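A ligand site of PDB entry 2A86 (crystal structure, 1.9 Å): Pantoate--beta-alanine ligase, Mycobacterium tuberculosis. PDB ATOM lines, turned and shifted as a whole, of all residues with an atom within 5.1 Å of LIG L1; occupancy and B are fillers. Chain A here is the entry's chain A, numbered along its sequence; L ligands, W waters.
OD1 of Asp 161 lies within salt-bridge range of N1 of LG2 L2 (3.9 Å). The backbone carbonyl oxygen of Gly 158 sits close to an oxygen (O7) of LIG L1 (3.4 Å). N3 of LIG L1 is in hydrogen-bond range of O of Met 195, 2.8 Å away. An oxygen (O6) of LIG L1 lies within hydrogen-bond range of the backbone NH (N) of Gly 158, at 3.0 Å. O of Val 187 lies within hydrogen-bond range of N3 of LIG L1 (3.0 Å). The backbone NH (N) of Met 40 is in hydrogen-bond range of an oxygen (O2) of LIG L1 (2.9 Å). The side-chain carboxylate of Asp 161 sits at hydrogen-bond distance from an oxygen (O7) of LIG L1 (2.7 Å). NE2 of His 47 is in hydrogen-bond range of O2 of LIG L1 (2.9 Å). A nitrogen (N4) of LIG L1 lies within hydrogen-bond range of the backbone NH (N) of Val 187 (2.9 Å).
O of Val 187 lies within hydrogen-bond range of N of Met 195, 3.0 Å away. The backbone NH (N) of Val 184 sits at hydrogen-bond distance from the backbone carbonyl oxygen (O) of Phe 157 (2.9 Å). The backbone NH of Lys 160 sits at hydrogen-bond distance from the side-chain hydroxyl of Thr 186 (2.9 Å). A ring nitrogen (ND1) of His 44 sits at hydrogen-bond distance from the backbone NH (N) of Gly 46 (3.0 Å). ND1 of His 47 is in hydrogen-bond range of N of His 44 (3.1 Å). NE2 of His 44 is in hydrogen-bond range of N of Ser 197. N of Gly 41 sits at hydrogen-bond distance from OG1 of Thr 39 (3.0 Å).
Merely in contact with LIG L1: Leu 50 (3.4 Å), Pro 38 (3.4 Å), His 44 (3.4 Å), Phe 157 (3.5 Å), Thr 186 (3.5 Å), Gly 46 (3.6 Å), Lys 160 (3.6 Å), Pro 185 (3.6 Å), Thr 39 (3.8 Å), Tyr 82 (3.8 Å) and Gln 164 (3.9 Å). Hydrophobic or aromatic side chains within 4 Å of LIG L1: Met 40, His 44, His 47, Leu 50, Phe 157, Val 187 and Met 195. 17 residues have an atom within 4 Å of LIG L1: Pro 38, Thr 39, Met 40, His 44, Gly 46, His 47, Leu 50, Tyr 82, Phe 157, Gly 158, Lys 160, Asp 161, Gln 164, Pro 185, Thr 186, Val 187 and Met 195. The nearest printed residue that does not touch LIG L1 is Val 184 (4.2 Å).
An oxygen (O3) of LIG L1 lies within hydrogen-bond range of a nitrogen (N1) of LG2 L2 (2.7 Å).
Water W2 lies within hydrogen-bond range of an oxygen (O1) of LIG L1 (2.5 Å), the side-chain hydroxyl (OH) of Tyr 82 (2.8 Å) and a nitrogen (N1) of LG2 L2 (3.1 Å). Water W3 lies within hydrogen-bond range of the backbone carbonyl oxygen (O) of Pro 38 (2.6 Å), an oxygen (O6) of LIG L1 (2.7 Å) and the backbone carbonyl oxygen (O) of Phe 156 (2.8 Å). Water W5 lies within hydrogen-bond range of the side-chain carboxylate (OD2) of Asp 161, an oxygen (O1) of LIG L1 and a nitrogen (N1) of LG2 L2. Water W6 lies within hydrogen-bond range of an oxygen (O1) of LIG L1 (2.8 Å), a ring nitrogen (NE2) of His 44 (2.9 Å) and the backbone NH of Ser 197 (2.9 Å). Water W1 lies within hydrogen-bond range of N2 of LIG L1 (3.1 Å), O of Met 195 (3.4 Å), OG of Ser 196 (3.5 Å) and NZ of Lys 160 (3.5 Å). Water W7 lies within hydrogen-bond range of the backbone carbonyl oxygen of Gly 158 (2.9 Å), the side-chain amide nitrogen of Gln 164 (3.0 Å), the backbone carbonyl oxygen of Asp 161 (3.1 Å) and an oxygen (O7) of LIG L1 (3.3 Å).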
ATOM      1  N   PRO A  38       3.348 -23.500   1.239  1.00  0.00           N
ATOM      2  CA  PRO A  38       3.687 -22.133   1.595  1.00  0.00           C
ATOM      3  C   PRO A  38       2.944 -21.144   0.724  1.00  0.00           C
ATOM      4  O   PRO A  38       2.976 -21.237  -0.516  1.00  0.00           O
ATOM      5  CB  PRO A  38       5.204 -22.050   1.323  1.00  0.00           C
ATOM      6  CG  PRO A  38       5.670 -23.524   1.413  1.00  0.00           C
ATOM      7  CD  PRO A  38       4.504 -24.229   0.669  1.00  0.00           C
ATOM      8  N   THR A  39       2.268 -20.210   1.388  1.00  0.00           N
ATOM      9  CA  THR A  39       1.629 -19.068   0.729  1.00  0.00           C
ATOM     10  C   THR A  39       1.853 -17.746   1.455  1.00  0.00           C
ATOM     11  O   THR A  39       2.309 -17.710   2.589  1.00  0.00           O
ATOM     12  CB  THR A  39       0.095 -19.240   0.573  1.00  0.00           C
ATOM     13  OG1 THR A  39      -0.576 -18.893   1.813  1.00  0.00           O
ATOM     14  CG2 THR A  39      -0.279 -20.741   0.352  1.00  0.00           C
ATOM     15  N   MET A  40       1.556 -16.679   0.736  1.00  0.00           N
ATOM     16  CA  MET A  40       1.466 -15.364   1.336  1.00  0.00           C
ATOM     17  C   MET A  40       0.026 -14.908   1.501  1.00  0.00           C
ATOM     18  O   MET A  40      -0.247 -13.729   1.589  1.00  0.00           O
ATOM     19  CB  MET A  40       2.291 -14.398   0.510  1.00  0.00           C
ATOM     20  CG  MET A  40       3.792 -14.846   0.550  1.00  0.00           C
ATOM     21  SD  MET A  40       4.925 -13.414   0.350  1.00  0.00           S
ATOM     22  CE  MET A  40       4.536 -12.950  -1.288  1.00  0.00           C
ATOM     23  N   GLY A  41      -0.877 -15.870   1.616  1.00  0.00           N
ATOM     24  CA  GLY A  41      -2.303 -15.523   1.736  1.00  0.00           C
ATOM     25  C   GLY A  41      -2.978 -14.861   0.539  1.00  0.00           C
ATOM     26  O   GLY A  41      -2.483 -14.933  -0.597  1.00  0.00           O
ATOM     27  N   HIS A  44      -6.500 -17.714  -3.703  1.00  0.00           N
ATOM     28  CA  HIS A  44      -7.355 -17.848  -4.866  1.00  0.00           C
ATOM     29  C   HIS A  44      -7.201 -19.290  -5.390  1.00  0.00           C
ATOM     30  O   HIS A  44      -6.533 -20.136  -4.754  1.00  0.00           O
ATOM     31  CB  HIS A  44      -6.946 -16.774  -5.913  1.00  0.00           C
ATOM     32  CG  HIS A  44      -5.486 -16.796  -6.268  1.00  0.00           C
ATOM     33  ND1 HIS A  44      -4.902 -17.846  -6.949  1.00  0.00           N
ATOM     34  CD2 HIS A  44      -4.480 -15.931  -5.992  1.00  0.00           C
ATOM     35  CE1 HIS A  44      -3.613 -17.621  -7.084  1.00  0.00           C
ATOM     36  NE2 HIS A  44      -3.325 -16.466  -6.511  1.00  0.00           N
ATOM     37  N   GLY A  46      -5.588 -20.654  -7.699  1.00  0.00           N
ATOM     38  CA  GLY A  46      -4.222 -21.093  -7.929  1.00  0.00           C
ATOM     39  C   GLY A  46      -3.636 -21.764  -6.678  1.00  0.00           C
ATOM     40  O   GLY A  46      -3.053 -22.869  -6.730  1.00  0.00           O
ATOM     41  N   HIS A  47      -3.816 -21.105  -5.543  1.00  0.00           N
ATOM     42  CA  HIS A  47      -3.378 -21.663  -4.266  1.00  0.00           C
ATOM     43  C   HIS A  47      -4.158 -22.929  -4.022  1.00  0.00           C
ATOM     44  O   HIS A  47      -3.575 -23.892  -3.545  1.00  0.00           O
ATOM     45  CB  HIS A  47      -3.652 -20.711  -3.116  1.00  0.00           C
ATOM     46  CG  HIS A  47      -2.863 -19.423  -3.184  1.00  0.00           C
ATOM     47  ND1 HIS A  47      -3.459 -18.198  -3.430  1.00  0.00           N
ATOM     48  CD2 HIS A  47      -1.529 -19.185  -3.065  1.00  0.00           C
ATOM     49  CE1 HIS A  47      -2.536 -17.254  -3.392  1.00  0.00           C
ATOM     50  NE2 HIS A  47      -1.357 -17.816  -3.180  1.00  0.00           N
ATOM     51  N   LEU A  50      -2.753 -26.168  -5.356  1.00  0.00           N
ATOM     52  CA  LEU A  50      -1.668 -26.751  -4.521  1.00  0.00           C
ATOM     53  C   LEU A  50      -2.260 -27.484  -3.295  1.00  0.00           C
ATOM     54  O   LEU A  50      -1.829 -28.609  -2.969  1.00  0.00           O
ATOM     55  CB  LEU A  50      -0.710 -25.636  -4.025  1.00  0.00           C
ATOM     56  CG  LEU A  50       0.417 -25.201  -4.977  1.00  0.00           C
ATOM     57  CD1 LEU A  50      -0.137 -24.516  -6.241  1.00  0.00           C
ATOM     58  CD2 LEU A  50       1.447 -24.310  -4.274  1.00  0.00           C
ATOM     59  N   TYR A  82       0.986  -5.255   0.060  1.00  0.00           N
ATOM     60  CA  TYR A  82       0.599  -6.632  -0.272  1.00  0.00           C
ATOM     61  C   TYR A  82      -0.819  -6.924   0.260  1.00  0.00           C
ATOM     62  O   TYR A  82      -1.135  -6.522   1.384  1.00  0.00           O
ATOM     63  CB  TYR A  82       1.595  -7.679   0.296  1.00  0.00           C
ATOM     64  CG  TYR A  82       1.447  -8.959  -0.482  1.00  0.00           C
ATOM     65  CD1 TYR A  82       2.072  -9.086  -1.734  1.00  0.00           C
ATOM     66  CD2 TYR A  82       0.660 -10.037  -0.005  1.00  0.00           C
ATOM     67  CE1 TYR A  82       1.884 -10.220  -2.521  1.00  0.00           C
ATOM     68  CE2 TYR A  82       0.478 -11.191  -0.792  1.00  0.00           C
ATOM     69  CZ  TYR A  82       1.086 -11.281  -2.029  1.00  0.00           C
ATOM     70  OH  TYR A  82       0.917 -12.421  -2.766  1.00  0.00           O
ATOM     71  N   PHE A 156       4.840 -28.118  -1.680  1.00  0.00           N
ATOM     72  CA  PHE A 156       4.124 -27.852  -2.946  1.00  0.00           C
ATOM     73  C   PHE A 156       4.403 -26.402  -3.384  1.00  0.00           C
ATOM     74  O   PHE A 156       4.218 -25.478  -2.578  1.00  0.00           O
ATOM     75  CB  PHE A 156       2.615 -28.129  -2.792  1.00  0.00           C
ATOM     76  CG  PHE A 156       2.323 -29.576  -2.584  1.00  0.00           C
ATOM     77  CD1 PHE A 156       2.546 -30.176  -1.319  1.00  0.00           C
ATOM     78  CD2 PHE A 156       2.023 -30.407  -3.672  1.00  0.00           C
ATOM     79  CE1 PHE A 156       2.377 -31.589  -1.144  1.00  0.00           C
ATOM     80  CE2 PHE A 156       1.803 -31.794  -3.492  1.00  0.00           C
ATOM     81  CZ  PHE A 156       2.007 -32.386  -2.242  1.00  0.00           C
ATOM     82  N   PHE A 157       4.877 -26.220  -4.621  1.00  0.00           N
ATOM     83  CA  PHE A 157       5.097 -24.907  -5.208  1.00  0.00           C
ATOM     84  C   PHE A 157       4.479 -24.848  -6.615  1.00  0.00           C
ATOM     85  O   PHE A 157       4.522 -25.840  -7.366  1.00  0.00           O
ATOM     86  CB  PHE A 157       6.606 -24.594  -5.283  1.00  0.00           C
ATOM     87  CG  PHE A 157       7.207 -24.181  -3.949  1.00  0.00           C
ATOM     88  CD1 PHE A 157       7.791 -25.137  -3.112  1.00  0.00           C
ATOM     89  CD2 PHE A 157       7.160 -22.853  -3.534  1.00  0.00           C
ATOM     90  CE1 PHE A 157       8.344 -24.779  -1.868  1.00  0.00           C
ATOM     91  CE2 PHE A 157       7.703 -22.479  -2.274  1.00  0.00           C
ATOM     92  CZ  PHE A 157       8.285 -23.422  -1.464  1.00  0.00           C
ATOM     93  N   GLY A 158       3.918 -23.682  -6.971  1.00  0.00           N
ATOM     94  CA  GLY A 158       3.314 -23.485  -8.299  1.00  0.00           C
ATOM     95  C   GLY A 158       4.339 -23.281  -9.407  1.00  0.00           C
ATOM     96  O   GLY A 158       5.349 -22.605  -9.235  1.00  0.00           O
ATOM     97  N   GLU A 159       4.071 -23.854 -10.573  1.00  0.00           N
ATOM     98  CA  GLU A 159       4.850 -23.506 -11.744  1.00  0.00           C
ATOM     99  C   GLU A 159       4.677 -22.045 -12.114  1.00  0.00           C
ATOM    100  O   GLU A 159       5.464 -21.507 -12.877  1.00  0.00           O
ATOM    101  CB  GLU A 159       4.425 -24.347 -12.929  1.00  0.00           C
ATOM    102  CG  GLU A 159       4.841 -25.815 -12.730  1.00  0.00           C
ATOM    103  CD  GLU A 159       4.566 -26.623 -13.979  1.00  0.00           C
ATOM    104  OE1 GLU A 159       4.114 -26.057 -14.997  1.00  0.00           O
ATOM    105  OE2 GLU A 159       4.824 -27.808 -13.917  1.00  0.00           O
ATOM    106  N   LYS A 160       3.602 -21.424 -11.638  1.00  0.00           N
ATOM    107  CA  LYS A 160       3.399 -19.976 -11.820  1.00  0.00           C
ATOM    108  C   LYS A 160       4.661 -19.144 -11.492  1.00  0.00           C
ATOM    109  O   LYS A 160       5.072 -18.257 -12.228  1.00  0.00           O
ATOM    110  CB  LYS A 160       2.193 -19.513 -10.970  1.00  0.00           C
ATOM    111  CG  LYS A 160       2.019 -17.986 -10.855  1.00  0.00           C
ATOM    112  CD  LYS A 160       1.445 -17.419 -12.100  1.00  0.00           C
ATOM    113  CE  LYS A 160       0.941 -15.963 -11.883  1.00  0.00           C
ATOM    114  NZ  LYS A 160       2.020 -15.079 -11.463  1.00  0.00           N
ATOM    115  N   ASP A 161       5.296 -19.459 -10.369  1.00  0.00           N
ATOM    116  CA  ASP A 161       6.526 -18.819  -9.992  1.00  0.00           C
ATOM    117  C   ASP A 161       7.636 -19.790 -10.303  1.00  0.00           C
ATOM    118  O   ASP A 161       8.188 -20.408  -9.431  1.00  0.00           O
ATOM    119  CB  ASP A 161       6.472 -18.453  -8.519  1.00  0.00           C
ATOM    120  CG  ASP A 161       5.310 -17.509  -8.239  1.00  0.00           C
ATOM    121  OD1 ASP A 161       5.481 -16.324  -8.507  1.00  0.00           O
ATOM    122  OD2 ASP A 161       4.190 -17.883  -7.835  1.00  0.00           O
ATOM    123  N   GLN A 164      11.185 -19.275  -8.859  1.00  0.00           N
ATOM    124  CA  GLN A 164      11.109 -19.652  -7.452  1.00  0.00           C
ATOM    125  C   GLN A 164      11.171 -21.168  -7.252  1.00  0.00           C
ATOM    126  O   GLN A 164      11.918 -21.663  -6.412  1.00  0.00           O
ATOM    127  CB  GLN A 164       9.777 -19.130  -6.879  1.00  0.00           C
ATOM    128  CG  GLN A 164       9.533 -19.652  -5.504  1.00  0.00           C
ATOM    129  CD  GLN A 164       8.434 -18.849  -4.818  1.00  0.00           C
ATOM    130  OE1 GLN A 164       8.705 -17.775  -4.237  1.00  0.00           O
ATOM    131  NE2 GLN A 164       7.225 -19.342  -4.921  1.00  0.00           N
ATOM    132  N   VAL A 184       3.344 -27.734  -9.171  1.00  0.00           N
ATOM    133  CA  VAL A 184       1.922 -27.810  -9.533  1.00  0.00           C
ATOM    134  C   VAL A 184       1.657 -26.845 -10.711  1.00  0.00           C
ATOM    135  O   VAL A 184       2.035 -25.663 -10.636  1.00  0.00           O
ATOM    136  CB  VAL A 184       1.055 -27.447  -8.321  1.00  0.00           C
ATOM    137  CG1 VAL A 184      -0.466 -27.485  -8.684  1.00  0.00           C
ATOM    138  CG2 VAL A 184       1.308 -28.445  -7.149  1.00  0.00           C
ATOM    139  N   PRO A 185       1.002 -27.348 -11.770  1.00  0.00           N
ATOM    140  CA  PRO A 185       0.741 -26.562 -12.981  1.00  0.00           C
ATOM    141  C   PRO A 185      -0.044 -25.299 -12.739  1.00  0.00           C
ATOM    142  O   PRO A 185      -0.898 -25.242 -11.834  1.00  0.00           O
ATOM    143  CB  PRO A 185      -0.094 -27.516 -13.845  1.00  0.00           C
ATOM    144  CG  PRO A 185       0.398 -28.840 -13.436  1.00  0.00           C
ATOM    145  CD  PRO A 185       0.483 -28.719 -11.910  1.00  0.00           C
ATOM    146  N   THR A 186       0.262 -24.283 -13.523  1.00  0.00           N
ATOM    147  CA  THR A 186      -0.355 -22.973 -13.362  1.00  0.00           C
ATOM    148  C   THR A 186      -1.883 -22.968 -13.620  1.00  0.00           C
ATOM    149  O   THR A 186      -2.391 -23.473 -14.619  1.00  0.00           O
ATOM    150  CB  THR A 186       0.354 -22.010 -14.293  1.00  0.00           C
ATOM    151  OG1 THR A 186       1.723 -21.840 -13.843  1.00  0.00           O
ATOM    152  CG2 THR A 186      -0.290 -20.608 -14.213  1.00  0.00           C
ATOM    153  N   VAL A 187      -2.595 -22.394 -12.673  1.00  0.00           N
ATOM    154  CA  VAL A 187      -4.048 -22.255 -12.755  1.00  0.00           C
ATOM    155  C   VAL A 187      -4.359 -20.962 -13.460  1.00  0.00           C
ATOM    156  O   VAL A 187      -3.807 -19.934 -13.067  1.00  0.00           O
ATOM    157  CB  VAL A 187      -4.755 -22.314 -11.346  1.00  0.00           C
ATOM    158  CG1 VAL A 187      -6.259 -22.153 -11.536  1.00  0.00           C
ATOM    159  CG2 VAL A 187      -4.463 -23.609 -10.652  1.00  0.00           C
ATOM    160  N   ALA A 194      -3.030 -16.109 -16.021  1.00  0.00           N
ATOM    161  CA  ALA A 194      -2.510 -16.850 -14.842  1.00  0.00           C
ATOM    162  C   ALA A 194      -3.103 -16.209 -13.585  1.00  0.00           C
ATOM    163  O   ALA A 194      -3.012 -14.995 -13.439  1.00  0.00           O
ATOM    164  CB  ALA A 194      -1.008 -16.757 -14.780  1.00  0.00           C
ATOM    165  N   MET A 195      -3.708 -17.003 -12.696  1.00  0.00           N
ATOM    166  CA  MET A 195      -4.272 -16.429 -11.479  1.00  0.00           C
ATOM    167  C   MET A 195      -3.175 -15.901 -10.578  1.00  0.00           C
ATOM    168  O   MET A 195      -2.132 -16.543 -10.450  1.00  0.00           O
ATOM    169  CB  MET A 195      -5.115 -17.456 -10.750  1.00  0.00           C
ATOM    170  CG  MET A 195      -6.432 -17.651 -11.506  1.00  0.00           C
ATOM    171  SD  MET A 195      -7.502 -18.641 -10.538  1.00  0.00           S
ATOM    172  CE  MET A 195      -8.866 -18.900 -11.646  1.00  0.00           C
ATOM    173  N   SER A 196      -3.399 -14.751  -9.965  1.00  0.00           N
ATOM    174  CA  SER A 196      -2.420 -14.199  -9.012  1.00  0.00           C
ATOM    175  C   SER A 196      -3.155 -13.261  -8.081  1.00  0.00           C
ATOM    176  O   SER A 196      -4.159 -12.643  -8.481  1.00  0.00           O
ATOM    177  CB  SER A 196      -1.422 -13.349  -9.805  1.00  0.00           C
ATOM    178  OG  SER A 196      -0.773 -12.386  -8.987  1.00  0.00           O
ATOM    179  N   SER A 197      -2.635 -13.107  -6.860  1.00  0.00           N
ATOM    180  CA  SER A 197      -3.236 -12.162  -5.876  1.00  0.00           C
ATOM    181  C   SER A 197      -3.103 -10.724  -6.383  1.00  0.00           C
ATOM    182  O   SER A 197      -3.872  -9.841  -5.978  1.00  0.00           O
ATOM    183  CB  SER A 197      -2.537 -12.304  -4.517  1.00  0.00           C
ATOM    184  OG  SER A 197      -2.668 -13.653  -4.023  1.00  0.00           O
HETATM  185  P1  LIG L   1       2.023 -16.614  -3.350  1.00  0.00           P
HETATM  186  O1  LIG L   1       1.576 -15.740  -4.489  1.00  0.00           O
HETATM  187  O2  LIG L   1       1.103 -16.650  -2.148  1.00  0.00           O
HETATM  188  O3  LIG L   1       3.466 -16.381  -2.983  1.00  0.00           O
HETATM  189  O4  LIG L   1       1.918 -18.106  -3.953  1.00  0.00           O
HETATM  190  C1  LIG L   1       2.031 -19.203  -3.033  1.00  0.00           C
HETATM  191  C2  LIG L   1       2.275 -20.474  -3.829  1.00  0.00           C
HETATM  192  O5  LIG L   1       1.150 -20.723  -4.682  1.00  0.00           O
HETATM  193  C3  LIG L   1       3.481 -20.333  -4.761  1.00  0.00           C
HETATM  194  O6  LIG L   1       4.031 -21.642  -4.799  1.00  0.00           O
HETATM  195  C4  LIG L   1       2.863 -20.019  -6.122  1.00  0.00           C
HETATM  196  O7  LIG L   1       3.644 -20.426  -7.261  1.00  0.00           O
HETATM  197  C5  LIG L   1       1.561 -20.768  -6.055  1.00  0.00           C
HETATM  198  N1  LIG L   1       0.648 -20.104  -6.996  1.00  0.00           N
HETATM  199  C6  LIG L   1       0.249 -18.795  -7.028  1.00  0.00           C
HETATM  200  N2  LIG L   1      -0.546 -18.573  -8.113  1.00  0.00           N
HETATM  201  C7  LIG L   1      -0.674 -19.754  -8.769  1.00  0.00           C
HETATM  202  C8  LIG L   1      -1.378 -20.238  -9.948  1.00  0.00           C
HETATM  203  N3  LIG L   1      -2.111 -19.379 -10.692  1.00  0.00           N
HETATM  204  N4  LIG L   1      -1.241 -21.554 -10.305  1.00  0.00           N
HETATM  205  C9  LIG L   1      -0.464 -22.419  -9.604  1.00  0.00           C
HETATM  206  N5  LIG L   1       0.203 -22.038  -8.496  1.00  0.00           N
HETATM  207  C10 LIG L   1       0.128 -20.751  -8.050  1.00  0.00           C
HETATM  208  N1  LG2 L   2       4.630 -15.011  -4.970  1.00  0.00           N
HETATM  209  C1  LG2 L   2       6.103 -15.229  -5.107  1.00  0.00           C
HETATM  210  C2  LG2 L   2       6.873 -14.395  -4.103  1.00  0.00           C
HETATM  211  C3  LG2 L   2       6.552 -12.910  -4.124  1.00  0.00           C
HETATM  212  O1  LG2 L   2       7.057 -12.136  -3.242  1.00  0.00           O
HETATM  213  O2  LG2 L   2       5.774 -12.517  -5.028  1.00  0.00           O
HETATM  214  O   HOH W   1       0.420 -15.598  -8.421  1.00  0.00           O
HETATM  215  O   HOH W   2       2.051 -13.334  -5.116  1.00  0.00           O
HETATM  216  O   HOH W   3       4.139 -22.723  -2.374  1.00  0.00           O
HETATM  217  O   HOH W   4      -0.497 -14.483  -2.152  1.00  0.00           O
HETATM  218  O   HOH W   5       2.498 -16.223  -6.989  1.00  0.00           O
HETATM  219  O   HOH W   6      -0.871 -15.137  -5.767  1.00  0.00           O
HETATM  220  O   HOH W   7       6.760 -21.506  -6.963  1.00  0.00           O
